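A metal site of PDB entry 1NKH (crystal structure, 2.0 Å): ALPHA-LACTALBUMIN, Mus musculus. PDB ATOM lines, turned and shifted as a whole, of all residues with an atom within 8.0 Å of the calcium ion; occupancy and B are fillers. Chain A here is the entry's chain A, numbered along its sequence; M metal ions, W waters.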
ATOM      1  N   THR A  38      -2.168   2.990  18.574  1.00  0.00           N
ATOM      2  CA  THR A  38      -1.364   2.447  17.475  1.00  0.00           C
ATOM      3  C   THR A  38      -0.041   1.832  17.930  1.00  0.00           C
ATOM      4  O   THR A  38       0.621   1.128  17.174  1.00  0.00           O
ATOM      5  CB  THR A  38      -1.065   3.524  16.448  1.00  0.00           C
ATOM      6  OG1 THR A  38      -0.220   4.524  17.040  1.00  0.00           O
ATOM      7  CG2 THR A  38      -2.358   4.169  15.948  1.00  0.00           C
ATOM      8  N   GLY A  51      -0.109  -3.050  17.671  1.00  0.00           N
ATOM      9  CA  GLY A  51      -0.902  -1.939  17.199  1.00  0.00           C
ATOM     10  C   GLY A  51      -2.390  -1.900  17.391  1.00  0.00           C
ATOM     11  O   GLY A  51      -2.964  -2.639  18.178  1.00  0.00           O
ATOM     12  N   ILE A  75       4.793  -8.705   6.645  1.00  0.00           N
ATOM     13  CA  ILE A  75       5.231  -7.403   7.117  1.00  0.00           C
ATOM     14  C   ILE A  75       5.918  -7.584   8.433  1.00  0.00           C
ATOM     15  O   ILE A  75       5.692  -8.564   9.137  1.00  0.00           O
ATOM     16  CB  ILE A  75       4.051  -6.431   7.347  1.00  0.00           C
ATOM     17  CG1 ILE A  75       3.173  -6.953   8.471  1.00  0.00           C
ATOM     18  CG2 ILE A  75       3.271  -6.213   6.043  1.00  0.00           C
ATOM     19  CD1 ILE A  75       1.945  -6.083   8.742  1.00  0.00           C
ATOM     20  N   SER A  76       6.765  -6.626   8.777  1.00  0.00           N
ATOM     21  CA  SER A  76       7.463  -6.664  10.047  1.00  0.00           C
ATOM     22  C   SER A  76       6.472  -6.147  11.101  1.00  0.00           C
ATOM     23  O   SER A  76       5.865  -5.079  10.938  1.00  0.00           O
ATOM     24  CB  SER A  76       8.685  -5.747   9.984  1.00  0.00           C
ATOM     25  OG  SER A  76       9.339  -5.712  11.236  1.00  0.00           O
ATOM     26  N   CYS A  77       6.284  -6.918  12.175  1.00  0.00           N
ATOM     27  CA  CYS A  77       5.366  -6.497  13.222  1.00  0.00           C
ATOM     28  C   CYS A  77       5.552  -5.018  13.640  1.00  0.00           C
ATOM     29  O   CYS A  77       4.559  -4.325  13.938  1.00  0.00           O
ATOM     30  CB  CYS A  77       5.521  -7.403  14.442  1.00  0.00           C
ATOM     31  SG  CYS A  77       5.178  -9.184  14.182  1.00  0.00           S
ATOM     32  N   ASP A  78       6.800  -4.544  13.646  1.00  0.00           N
ATOM     33  CA  ASP A  78       7.095  -3.144  14.020  1.00  0.00           C
ATOM     34  C   ASP A  78       6.375  -2.133  13.140  1.00  0.00           C
ATOM     35  O   ASP A  78       6.172  -0.995  13.560  1.00  0.00           O
ATOM     36  CB  ASP A  78       8.585  -2.820  13.922  1.00  0.00           C
ATOM     37  CG  ASP A  78       9.409  -3.483  14.972  1.00  0.00           C
ATOM     38  OD1 ASP A  78       8.909  -3.667  16.107  1.00  0.00           O
ATOM     39  OD2 ASP A  78      10.576  -3.801  14.668  1.00  0.00           O
ATOM     40  N   LYS A  79       6.028  -2.515  11.930  1.00  0.00           N
ATOM     41  CA  LYS A  79       5.351  -1.573  11.046  1.00  0.00           C
ATOM     42  C   LYS A  79       3.879  -1.355  11.438  1.00  0.00           C
ATOM     43  O   LYS A  79       3.169  -0.559  10.819  1.00  0.00           O
ATOM     44  CB  LYS A  79       5.458  -2.029   9.600  1.00  0.00           C
ATOM     45  CG  LYS A  79       6.444  -1.198   8.756  1.00  0.00           C
ATOM     46  CD  LYS A  79       7.884  -1.360   9.222  1.00  0.00           C
ATOM     47  CE  LYS A  79       8.834  -0.464   8.422  1.00  0.00           C
ATOM     48  NZ  LYS A  79       8.479   0.971   8.623  1.00  0.00           N
ATOM     49  N   LEU A  80       3.448  -2.065  12.472  1.00  0.00           N
ATOM     50  CA  LEU A  80       2.087  -1.925  12.979  1.00  0.00           C
ATOM     51  C   LEU A  80       2.157  -1.099  14.293  1.00  0.00           C
ATOM     52  O   LEU A  80       1.179  -1.025  15.051  1.00  0.00           O
ATOM     53  CB  LEU A  80       1.469  -3.300  13.231  1.00  0.00           C
ATOM     54  CG  LEU A  80       1.524  -4.223  11.988  1.00  0.00           C
ATOM     55  CD1 LEU A  80       1.541  -5.689  12.436  1.00  0.00           C
ATOM     56  CD2 LEU A  80       0.365  -3.907  11.041  1.00  0.00           C
ATOM     57  N   LEU A  81       3.315  -0.485  14.539  1.00  0.00           N
ATOM     58  CA  LEU A  81       3.491   0.353  15.723  1.00  0.00           C
ATOM     59  C   LEU A  81       3.686   1.822  15.325  1.00  0.00           C
ATOM     60  O   LEU A  81       4.049   2.658  16.155  1.00  0.00           O
ATOM     61  CB  LEU A  81       4.666  -0.120  16.561  1.00  0.00           C
ATOM     62  CG  LEU A  81       4.506  -1.557  17.082  1.00  0.00           C
ATOM     63  CD1 LEU A  81       5.766  -1.996  17.751  1.00  0.00           C
ATOM     64  CD2 LEU A  81       3.358  -1.660  18.046  1.00  0.00           C
ATOM     65  N   ASP A  82       3.463   2.147  14.054  1.00  0.00           N
ATOM     66  CA  ASP A  82       3.620   3.536  13.637  1.00  0.00           C
ATOM     67  C   ASP A  82       2.222   4.064  13.379  1.00  0.00           C
ATOM     68  O   ASP A  82       1.262   3.359  13.613  1.00  0.00           O
ATOM     69  CB  ASP A  82       4.494   3.663  12.384  1.00  0.00           C
ATOM     70  CG  ASP A  82       3.859   3.069  11.148  1.00  0.00           C
ATOM     71  OD1 ASP A  82       2.636   3.210  10.967  1.00  0.00           O
ATOM     72  OD2 ASP A  82       4.596   2.483  10.330  1.00  0.00           O
ATOM     73  N   ASP A  83       2.113   5.282  12.880  1.00  0.00           N
ATOM     74  CA  ASP A  83       0.800   5.868  12.649  1.00  0.00           C
ATOM     75  C   ASP A  83       0.218   5.744  11.261  1.00  0.00           C
ATOM     76  O   ASP A  83      -0.816   6.349  10.973  1.00  0.00           O
ATOM     77  CB  ASP A  83       0.813   7.337  13.100  1.00  0.00           C
ATOM     78  CG  ASP A  83       0.904   7.489  14.625  1.00  0.00           C
ATOM     79  OD1 ASP A  83       1.388   6.556  15.303  1.00  0.00           O
ATOM     80  OD2 ASP A  83       0.490   8.543  15.145  1.00  0.00           O
ATOM     81  N   GLU A  84       0.872   4.972  10.381  1.00  0.00           N
ATOM     82  CA  GLU A  84       0.313   4.746   9.034  1.00  0.00           C
ATOM     83  C   GLU A  84      -0.386   3.396   9.126  1.00  0.00           C
ATOM     84  O   GLU A  84       0.261   2.347   9.263  1.00  0.00           O
ATOM     85  CB  GLU A  84       1.417   4.704   7.978  1.00  0.00           C
ATOM     86  CG  GLU A  84       1.871   6.075   7.525  1.00  0.00           C
ATOM     87  CD  GLU A  84       2.900   6.006   6.412  1.00  0.00           C
ATOM     88  OE1 GLU A  84       2.615   5.349   5.382  1.00  0.00           O
ATOM     89  OE2 GLU A  84       3.995   6.603   6.574  1.00  0.00           O
ATOM     90  N   LEU A  85      -1.709   3.431   9.077  1.00  0.00           N
ATOM     91  CA  LEU A  85      -2.522   2.227   9.236  1.00  0.00           C
ATOM     92  C   LEU A  85      -2.796   1.391   7.976  1.00  0.00           C
ATOM     93  O   LEU A  85      -3.390   0.306   8.081  1.00  0.00           O
ATOM     94  CB  LEU A  85      -3.854   2.622   9.907  1.00  0.00           C
ATOM     95  CG  LEU A  85      -3.911   2.712  11.445  1.00  0.00           C
ATOM     96  CD1 LEU A  85      -2.590   3.113  12.011  1.00  0.00           C
ATOM     97  CD2 LEU A  85      -4.978   3.730  11.856  1.00  0.00           C
ATOM     98  N   ASP A  86      -2.376   1.859   6.813  1.00  0.00           N
ATOM     99  CA  ASP A  86      -2.618   1.131   5.580  1.00  0.00           C
ATOM    100  C   ASP A  86      -2.177  -0.331   5.621  1.00  0.00           C
ATOM    101  O   ASP A  86      -2.925  -1.215   5.225  1.00  0.00           O
ATOM    102  CB  ASP A  86      -1.955   1.834   4.401  1.00  0.00           C
ATOM    103  CG  ASP A  86      -2.414   3.256   4.276  1.00  0.00           C
ATOM    104  OD1 ASP A  86      -1.955   4.100   5.096  1.00  0.00           O
ATOM    105  OD2 ASP A  86      -3.240   3.540   3.379  1.00  0.00           O
ATOM    106  N   ASP A  87      -0.968  -0.602   6.112  1.00  0.00           N
ATOM    107  CA  ASP A  87      -0.556  -1.998   6.173  1.00  0.00           C
ATOM    108  C   ASP A  87      -1.259  -2.769   7.291  1.00  0.00           C
ATOM    109  O   ASP A  87      -1.526  -3.962   7.151  1.00  0.00           O
ATOM    110  CB  ASP A  87       0.987  -2.138   6.265  1.00  0.00           C
ATOM    111  CG  ASP A  87       1.646  -1.219   7.319  1.00  0.00           C
ATOM    112  OD1 ASP A  87       0.962  -0.614   8.170  1.00  0.00           O
ATOM    113  OD2 ASP A  87       2.883  -1.144   7.283  1.00  0.00           O
ATOM    114  N   ASP A  88      -1.588  -2.067   8.387  1.00  0.00           N
ATOM    115  CA  ASP A  88      -2.295  -2.697   9.505  1.00  0.00           C
ATOM    116  C   ASP A  88      -3.626  -3.176   8.933  1.00  0.00           C
ATOM    117  O   ASP A  88      -4.006  -4.331   9.077  1.00  0.00           O
ATOM    118  CB  ASP A  88      -2.540  -1.692  10.636  1.00  0.00           C
ATOM    119  CG  ASP A  88      -1.247  -1.028  11.150  1.00  0.00           C
ATOM    120  OD1 ASP A  88      -0.982  -1.067  12.364  1.00  0.00           O
ATOM    121  OD2 ASP A  88      -0.496  -0.458  10.323  1.00  0.00           O
ATOM    122  N   ILE A  89      -4.299  -2.276   8.223  1.00  0.00           N
ATOM    123  CA  ILE A  89      -5.581  -2.547   7.615  1.00  0.00           C
ATOM    124  C   ILE A  89      -5.494  -3.642   6.579  1.00  0.00           C
ATOM    125  O   ILE A  89      -6.387  -4.469   6.483  1.00  0.00           O
ATOM    126  CB  ILE A  89      -6.148  -1.292   6.914  1.00  0.00           C
ATOM    127  CG1 ILE A  89      -6.459  -0.208   7.969  1.00  0.00           C
ATOM    128  CG2 ILE A  89      -7.404  -1.669   6.113  1.00  0.00           C
ATOM    129  CD1 ILE A  89      -7.016   1.078   7.387  1.00  0.00           C
HETATM  130 CA    CA M   1       1.558   0.732  10.109  1.00  0.00          CA
HETATM  131  O   HOH W   1       3.257   1.232   8.226  1.00  0.00           O
HETATM  132  O   HOH W   2       0.974   1.110  12.582  1.00  0.00           O
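Merely in contact with the calcium ion: Leu 80 (3.9 Å).
Of the 17 residues printed, 6 come within 4 Å of the calcium ion.
The nearest printed residue that does not touch the calcium ion is Leu 85 (4.4 Å).
Water W1 bridges OD2 of Asp 87 and OD2 of Asp 82.
The calcium ion is bound by O of Lys 79, at 2.2 Å.
The calcium ion is bound by O of Glu 84, at 2.2 Å.
OD2 of Asp 88 binds the calcium ion (2.4 Å).
OD1 of Asp 87 binds the calcium ion (2.4 Å).
Water W2 binds the calcium ion (2.6 Å).
Water W1 is bound to the calcium ion (2.6 Å).
The side-chain carboxylate (OD1) of Asp 82 binds the calcium ion (2.8 Å).
The calcium ion has seven donor atoms within binding distance.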
